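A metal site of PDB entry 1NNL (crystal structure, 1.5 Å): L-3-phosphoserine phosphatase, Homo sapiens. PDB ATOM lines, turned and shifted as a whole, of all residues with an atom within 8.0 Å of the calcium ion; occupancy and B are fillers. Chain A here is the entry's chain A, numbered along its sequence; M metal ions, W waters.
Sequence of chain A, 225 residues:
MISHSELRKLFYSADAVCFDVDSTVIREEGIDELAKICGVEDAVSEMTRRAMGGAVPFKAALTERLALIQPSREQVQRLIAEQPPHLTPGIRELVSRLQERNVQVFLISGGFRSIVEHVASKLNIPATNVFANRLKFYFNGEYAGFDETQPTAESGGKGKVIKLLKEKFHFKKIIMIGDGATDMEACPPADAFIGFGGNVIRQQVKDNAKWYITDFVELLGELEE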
ATOM      1  N   PHE A  19     -20.018  -8.934   2.155  1.00  0.00           N
ATOM      2  CA  PHE A  19     -21.026  -9.241   1.154  1.00  0.00           C
ATOM      3  C   PHE A  19     -22.102 -10.168   1.661  1.00  0.00           C
ATOM      4  O   PHE A  19     -21.836 -11.160   2.337  1.00  0.00           O
ATOM      5  CB  PHE A  19     -20.424  -9.971  -0.042  1.00  0.00           C
ATOM      6  CG  PHE A  19     -19.512  -9.147  -0.893  1.00  0.00           C
ATOM      7  CD1 PHE A  19     -18.132  -9.152  -0.667  1.00  0.00           C
ATOM      8  CD2 PHE A  19     -20.006  -8.412  -1.962  1.00  0.00           C
ATOM      9  CE1 PHE A  19     -17.276  -8.441  -1.498  1.00  0.00           C
ATOM     10  CE2 PHE A  19     -19.164  -7.697  -2.802  1.00  0.00           C
ATOM     11  CZ  PHE A  19     -17.796  -7.714  -2.575  1.00  0.00           C
ATOM     12  N   ASP A  20     -23.331  -9.823   1.305  1.00  0.00           N
ATOM     13  CA  ASP A  20     -24.494 -10.667   1.572  1.00  0.00           C
ATOM     14  C   ASP A  20     -24.288 -11.784   0.545  1.00  0.00           C
ATOM     15  O   ASP A  20     -23.658 -11.558  -0.510  1.00  0.00           O
ATOM     16  CB  ASP A  20     -25.754  -9.847   1.282  1.00  0.00           C
ATOM     17  CG  ASP A  20     -26.950 -10.694   0.883  1.00  0.00           C
ATOM     18  OD1 ASP A  20     -27.389 -10.558  -0.273  1.00  0.00           O
ATOM     19  OD2 ASP A  20     -27.452 -11.467   1.722  1.00  0.00           O
ATOM     20  N   VAL A  21     -24.784 -12.981   0.804  1.00  0.00           N
ATOM     21  CA  VAL A  21     -24.597 -14.085  -0.134  1.00  0.00           C
ATOM     22  C   VAL A  21     -25.740 -14.285  -1.119  1.00  0.00           C
ATOM     23  O   VAL A  21     -25.568 -14.081  -2.324  1.00  0.00           O
ATOM     24  CB  VAL A  21     -24.322 -15.408   0.609  1.00  0.00           C
ATOM     25  CG1 VAL A  21     -24.141 -16.548  -0.392  1.00  0.00           C
ATOM     26  CG2 VAL A  21     -23.062 -15.266   1.465  1.00  0.00           C
ATOM     27  N   ASP A  22     -26.919 -14.666  -0.607  1.00  0.00           N
ATOM     28  CA  ASP A  22     -28.079 -14.930  -1.455  1.00  0.00           C
ATOM     29  C   ASP A  22     -28.526 -13.711  -2.258  1.00  0.00           C
ATOM     30  O   ASP A  22     -28.886 -12.672  -1.695  1.00  0.00           O
ATOM     31  CB  ASP A  22     -29.259 -15.426  -0.618  1.00  0.00           C
ATOM     32  CG  ASP A  22     -28.994 -16.761   0.048  1.00  0.00           C
ATOM     33  OD1 ASP A  22     -28.011 -17.449  -0.318  1.00  0.00           O
ATOM     34  OD2 ASP A  22     -29.783 -17.131   0.949  1.00  0.00           O
ATOM     35  N   SER A  23     -28.507 -13.865  -3.585  1.00  0.00           N
ATOM     36  CA  SER A  23     -28.887 -12.839  -4.561  1.00  0.00           C
ATOM     37  C   SER A  23     -27.841 -11.755  -4.764  1.00  0.00           C
ATOM     38  O   SER A  23     -28.051 -10.834  -5.559  1.00  0.00           O
ATOM     39  CB  SER A  23     -30.244 -12.218  -4.201  1.00  0.00           C
ATOM     40  OG  SER A  23     -31.293 -13.149  -4.397  1.00  0.00           O
ATOM     41  N   THR A  24     -26.721 -11.842  -4.054  1.00  0.00           N
ATOM     42  CA  THR A  24     -25.653 -10.878  -4.230  1.00  0.00           C
ATOM     43  C   THR A  24     -24.420 -11.590  -4.779  1.00  0.00           C
ATOM     44  O   THR A  24     -24.106 -11.459  -5.963  1.00  0.00           O
ATOM     45  CB  THR A  24     -25.341 -10.142  -2.900  1.00  0.00           C
ATOM     46  OG1 THR A  24     -26.497  -9.405  -2.488  1.00  0.00           O
ATOM     47  CG2 THR A  24     -24.188  -9.169  -3.080  1.00  0.00           C
ATOM     48  N   VAL A  25     -23.733 -12.354  -3.929  1.00  0.00           N
ATOM     49  CA  VAL A  25     -22.557 -13.104  -4.367  1.00  0.00           C
ATOM     50  C   VAL A  25     -22.972 -14.277  -5.260  1.00  0.00           C
ATOM     51  O   VAL A  25     -22.239 -14.650  -6.170  1.00  0.00           O
ATOM     52  CB  VAL A  25     -21.742 -13.600  -3.162  1.00  0.00           C
ATOM     53  CG1 VAL A  25     -20.667 -14.593  -3.615  1.00  0.00           C
ATOM     54  CG2 VAL A  25     -21.081 -12.395  -2.474  1.00  0.00           C
ATOM     55  N   ILE A  26     -24.137 -14.845  -4.977  1.00  0.00           N
ATOM     56  CA  ILE A  26     -24.658 -15.934  -5.800  1.00  0.00           C
ATOM     57  C   ILE A  26     -26.026 -15.535  -6.332  1.00  0.00           C
ATOM     58  O   ILE A  26     -26.668 -14.633  -5.798  1.00  0.00           O
ATOM     59  CB  ILE A  26     -24.781 -17.271  -5.024  1.00  0.00           C
ATOM     60  CG1 ILE A  26     -25.742 -17.115  -3.850  1.00  0.00           C
ATOM     61  CG2 ILE A  26     -23.401 -17.725  -4.590  1.00  0.00           C
ATOM     62  CD1 ILE A  26     -26.006 -18.410  -3.088  1.00  0.00           C
ATOM     63  N   GLU A  28     -28.747 -17.606  -6.593  1.00  0.00           N
ATOM     64  CA  GLU A  28     -29.820 -18.250  -5.836  1.00  0.00           C
ATOM     65  C   GLU A  28     -29.882 -17.909  -4.356  1.00  0.00           C
ATOM     66  O   GLU A  28     -29.198 -17.015  -3.873  1.00  0.00           O
ATOM     67  CB  GLU A  28     -29.713 -19.778  -5.976  1.00  0.00           C
ATOM     68  CG  GLU A  28     -29.505 -20.256  -7.409  1.00  0.00           C
ATOM     69  CD  GLU A  28     -28.038 -20.476  -7.743  1.00  0.00           C
ATOM     70  OE1 GLU A  28     -27.193 -19.690  -7.263  1.00  0.00           O
ATOM     71  OE2 GLU A  28     -27.745 -21.425  -8.497  1.00  0.00           O
ATOM     72  N   GLU A  29     -30.742 -18.655  -3.666  1.00  0.00           N
ATOM     73  CA  GLU A  29     -30.936 -18.532  -2.229  1.00  0.00           C
ATOM     74  C   GLU A  29     -30.678 -19.919  -1.653  1.00  0.00           C
ATOM     75  O   GLU A  29     -31.429 -20.857  -1.913  1.00  0.00           O
ATOM     76  CB  GLU A  29     -32.373 -18.113  -1.920  1.00  0.00           C
ATOM     77  CG  GLU A  29     -32.707 -18.087  -0.436  1.00  0.00           C
ATOM     78  CD  GLU A  29     -34.190 -17.863  -0.173  1.00  0.00           C
ATOM     79  OE1 GLU A  29     -35.001 -18.710  -0.604  1.00  0.00           O
ATOM     80  OE2 GLU A  29     -34.536 -16.842   0.458  1.00  0.00           O
ATOM     81  N   ILE A 108     -21.537 -12.713   4.822  1.00  0.00           N
ATOM     82  CA  ILE A 108     -22.481 -12.802   5.929  1.00  0.00           C
ATOM     83  C   ILE A 108     -23.808 -13.266   5.358  1.00  0.00           C
ATOM     84  O   ILE A 108     -24.287 -12.705   4.367  1.00  0.00           O
ATOM     85  CB  ILE A 108     -22.696 -11.444   6.629  1.00  0.00           C
ATOM     86  CG1 ILE A 108     -21.346 -10.822   7.002  1.00  0.00           C
ATOM     87  CG2 ILE A 108     -23.535 -11.650   7.891  1.00  0.00           C
ATOM     88  CD1 ILE A 108     -21.458  -9.400   7.566  1.00  0.00           C
ATOM     89  N   SER A 109     -24.392 -14.290   5.962  1.00  0.00           N
ATOM     90  CA  SER A 109     -25.644 -14.811   5.457  1.00  0.00           C
ATOM     91  C   SER A 109     -26.515 -15.418   6.532  1.00  0.00           C
ATOM     92  O   SER A 109     -26.012 -15.907   7.542  1.00  0.00           O
ATOM     93  CB  SER A 109     -25.352 -15.868   4.392  1.00  0.00           C
ATOM     94  OG  SER A 109     -26.554 -16.421   3.860  1.00  0.00           O
ATOM     95  N   GLY A 110     -27.825 -15.368   6.309  1.00  0.00           N
ATOM     96  CA  GLY A 110     -28.766 -15.959   7.228  1.00  0.00           C
ATOM     97  C   GLY A 110     -28.889 -17.403   6.783  1.00  0.00           C
ATOM     98  O   GLY A 110     -29.667 -18.183   7.332  1.00  0.00           O
ATOM     99  N   LYS A 158     -26.659  -9.232  10.537  1.00  0.00           N
ATOM    100  CA  LYS A 158     -25.591  -8.665   9.729  1.00  0.00           C
ATOM    101  C   LYS A 158     -24.934  -7.502  10.445  1.00  0.00           C
ATOM    102  O   LYS A 158     -23.705  -7.403  10.482  1.00  0.00           O
ATOM    103  CB  LYS A 158     -26.126  -8.252   8.351  1.00  0.00           C
ATOM    104  CG  LYS A 158     -26.472  -9.469   7.506  1.00  0.00           C
ATOM    105  CD  LYS A 158     -27.193  -9.124   6.216  1.00  0.00           C
ATOM    106  CE  LYS A 158     -27.477 -10.401   5.432  1.00  0.00           C
ATOM    107  NZ  LYS A 158     -28.339 -10.166   4.249  1.00  0.00           N
ATOM    108  N   MET A 176     -20.925  -2.561   3.611  1.00  0.00           N
ATOM    109  CA  MET A 176     -21.820  -3.700   3.440  1.00  0.00           C
ATOM    110  C   MET A 176     -22.386  -3.626   2.025  1.00  0.00           C
ATOM    111  O   MET A 176     -22.793  -2.557   1.578  1.00  0.00           O
ATOM    112  CB  MET A 176     -22.973  -3.613   4.440  1.00  0.00           C
ATOM    113  CG  MET A 176     -24.014  -4.719   4.301  1.00  0.00           C
ATOM    114  SD  MET A 176     -23.458  -6.257   5.068  1.00  0.00           S
ATOM    115  CE  MET A 176     -23.969  -7.475   3.854  1.00  0.00           C
ATOM    116  N   ILE A 177     -22.387  -4.766   1.333  1.00  0.00           N
ATOM    117  CA  ILE A 177     -22.924  -4.832  -0.031  1.00  0.00           C
ATOM    118  C   ILE A 177     -23.959  -5.939  -0.071  1.00  0.00           C
ATOM    119  O   ILE A 177     -23.662  -7.094   0.252  1.00  0.00           O
ATOM    120  CB  ILE A 177     -21.811  -5.118  -1.064  1.00  0.00           C
ATOM    121  CG1 ILE A 177     -20.769  -4.001  -1.008  1.00  0.00           C
ATOM    122  CG2 ILE A 177     -22.412  -5.230  -2.471  1.00  0.00           C
ATOM    123  CD1 ILE A 177     -19.677  -4.090  -2.055  1.00  0.00           C
ATOM    124  N   GLY A 178     -25.184  -5.591  -0.444  1.00  0.00           N
ATOM    125  CA  GLY A 178     -26.227  -6.589  -0.474  1.00  0.00           C
ATOM    126  C   GLY A 178     -27.421  -6.096  -1.269  1.00  0.00           C
ATOM    127  O   GLY A 178     -27.498  -4.924  -1.637  1.00  0.00           O
ATOM    128  N   ASP A 179     -28.370  -6.994  -1.493  1.00  0.00           N
ATOM    129  CA  ASP A 179     -29.545  -6.681  -2.283  1.00  0.00           C
ATOM    130  C   ASP A 179     -30.778  -6.276  -1.500  1.00  0.00           C
ATOM    131  O   ASP A 179     -31.669  -5.623  -2.050  1.00  0.00           O
ATOM    132  CB  ASP A 179     -29.921  -7.880  -3.151  1.00  0.00           C
ATOM    133  CG  ASP A 179     -30.459  -9.034  -2.320  1.00  0.00           C
ATOM    134  OD1 ASP A 179     -31.594  -9.484  -2.568  1.00  0.00           O
ATOM    135  OD2 ASP A 179     -29.734  -9.502  -1.408  1.00  0.00           O
ATOM    136  N   GLY A 180     -30.852  -6.658  -0.226  1.00  0.00           N
ATOM    137  CA  GLY A 180     -32.064  -6.374   0.524  1.00  0.00           C
ATOM    138  C   GLY A 180     -32.045  -5.422   1.694  1.00  0.00           C
ATOM    139  O   GLY A 180     -31.035  -4.815   2.024  1.00  0.00           O
ATOM    140  N   ALA A 181     -33.214  -5.300   2.312  1.00  0.00           N
ATOM    141  CA  ALA A 181     -33.408  -4.422   3.447  1.00  0.00           C
ATOM    142  C   ALA A 181     -32.489  -4.765   4.610  1.00  0.00           C
ATOM    143  O   ALA A 181     -31.959  -3.872   5.250  1.00  0.00           O
ATOM    144  CB  ALA A 181     -34.869  -4.465   3.907  1.00  0.00           C
ATOM    145  N   THR A 182     -32.286  -6.057   4.859  1.00  0.00           N
ATOM    146  CA  THR A 182     -31.412  -6.448   5.971  1.00  0.00           C
ATOM    147  C   THR A 182     -29.987  -5.956   5.736  1.00  0.00           C
ATOM    148  O   THR A 182     -29.249  -5.671   6.682  1.00  0.00           O
ATOM    149  CB  THR A 182     -31.381  -7.990   6.190  1.00  0.00           C
ATOM    150  OG1 THR A 182     -30.941  -8.665   5.007  1.00  0.00           O
ATOM    151  CG2 THR A 182     -32.768  -8.493   6.580  1.00  0.00           C
ATOM    152  N   ASP A 183     -29.598  -5.826   4.469  1.00  0.00           N
ATOM    153  CA  ASP A 183     -28.258  -5.355   4.158  1.00  0.00           C
ATOM    154  C   ASP A 183     -28.169  -3.844   4.361  1.00  0.00           C
ATOM    155  O   ASP A 183     -27.204  -3.348   4.934  1.00  0.00           O
ATOM    156  CB  ASP A 183     -27.903  -5.724   2.717  1.00  0.00           C
ATOM    157  CG  ASP A 183     -28.041  -7.201   2.463  1.00  0.00           C
ATOM    158  OD1 ASP A 183     -27.299  -7.962   3.123  1.00  0.00           O
ATOM    159  OD2 ASP A 183     -28.874  -7.588   1.624  1.00  0.00           O
ATOM    160  N   PHE A 196     -27.202  -3.851  -4.232  1.00  0.00           N
ATOM    161  CA  PHE A 196     -26.908  -4.628  -5.437  1.00  0.00           C
ATOM    162  C   PHE A 196     -28.159  -5.227  -6.058  1.00  0.00           C
ATOM    163  O   PHE A 196     -28.865  -6.022  -5.431  1.00  0.00           O
ATOM    164  CB  PHE A 196     -25.940  -5.758  -5.112  1.00  0.00           C
ATOM    165  CG  PHE A 196     -25.531  -6.555  -6.318  1.00  0.00           C
ATOM    166  CD1 PHE A 196     -24.669  -6.003  -7.265  1.00  0.00           C
ATOM    167  CD2 PHE A 196     -26.040  -7.833  -6.520  1.00  0.00           C
ATOM    168  CE1 PHE A 196     -24.338  -6.710  -8.417  1.00  0.00           C
ATOM    169  CE2 PHE A 196     -25.712  -8.554  -7.676  1.00  0.00           C
ATOM    170  CZ  PHE A 196     -24.862  -7.984  -8.629  1.00  0.00           C
ATOM    171  N   ARG A 202     -34.489  -4.981  -5.696  1.00  0.00           N
ATOM    172  CA  ARG A 202     -35.467  -4.784  -4.629  1.00  0.00           C
ATOM    173  C   ARG A 202     -35.625  -3.278  -4.617  1.00  0.00           C
ATOM    174  O   ARG A 202     -34.754  -2.532  -4.174  1.00  0.00           O
ATOM    175  CB  ARG A 202     -34.944  -5.345  -3.304  1.00  0.00           C
ATOM    176  CG  ARG A 202     -34.973  -6.869  -3.323  1.00  0.00           C
ATOM    177  CD  ARG A 202     -34.415  -7.520  -2.083  1.00  0.00           C
ATOM    178  NE  ARG A 202     -34.497  -8.978  -2.196  1.00  0.00           N
ATOM    179  CZ  ARG A 202     -35.600  -9.692  -2.000  1.00  0.00           C
ATOM    180  NH1 ARG A 202     -36.742  -9.088  -1.662  1.00  0.00           N
ATOM    181  NH2 ARG A 202     -35.572 -11.009  -2.138  1.00  0.00           N
HETATM  182 CA    CA M   1     -29.626 -11.311   0.007  1.00  0.00          CA
HETATM  183  O   HOH W   1     -30.441 -13.003   1.569  1.00  0.00           O
HETATM  184  O   HOH W   2     -31.809 -11.640  -0.827  1.00  0.00           O
HETATM  185  O   HOH W   3     -30.252  -9.865   1.732  1.00  0.00           O
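OD1 of Asp 179 lies within salt-bridge range of NE of Arg 202, at 3.0 Å.
The side-chain amino group of Lys 158 lies close to the side-chain carboxylate of Asp 20 (3.0 Å).
The side-chain hydroxyl (OG1) of Thr 24 is in hydrogen-bond range of the backbone NH (N) of Asp 179, 3.2 Å away.
The backbone NH of Asp 20 lies within hydrogen-bond range of the backbone carbonyl oxygen of Ile 177, 2.9 Å away.
OD2 of Asp 183 sits at hydrogen-bond distance from N of Asp 179.
The side-chain carboxylate of Asp 20 sits close to the side-chain hydroxyl of Thr 24, at 2.7 Å.
Of the 24 residues printed, 3 come within 4 Å of the calcium ion.
The calcium ion is bound by the side-chain carboxylate (OD2) of Asp 179 (2.3 Å), the backbone carbonyl oxygen (O) of Asp 22 (2.3 Å), water W3 (2.3 Å), water W2 (2.4 Å), the side-chain carboxylate (OD1) of Asp 20 (2.4 Å), water W1 (2.4 Å) and the side-chain carboxylate (OD2) of Asp 20 (2.8 Å).
Water W3 lies within hydrogen-bond range of the side-chain carboxylate of Asp 183 and the side-chain amino group of Lys 158.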
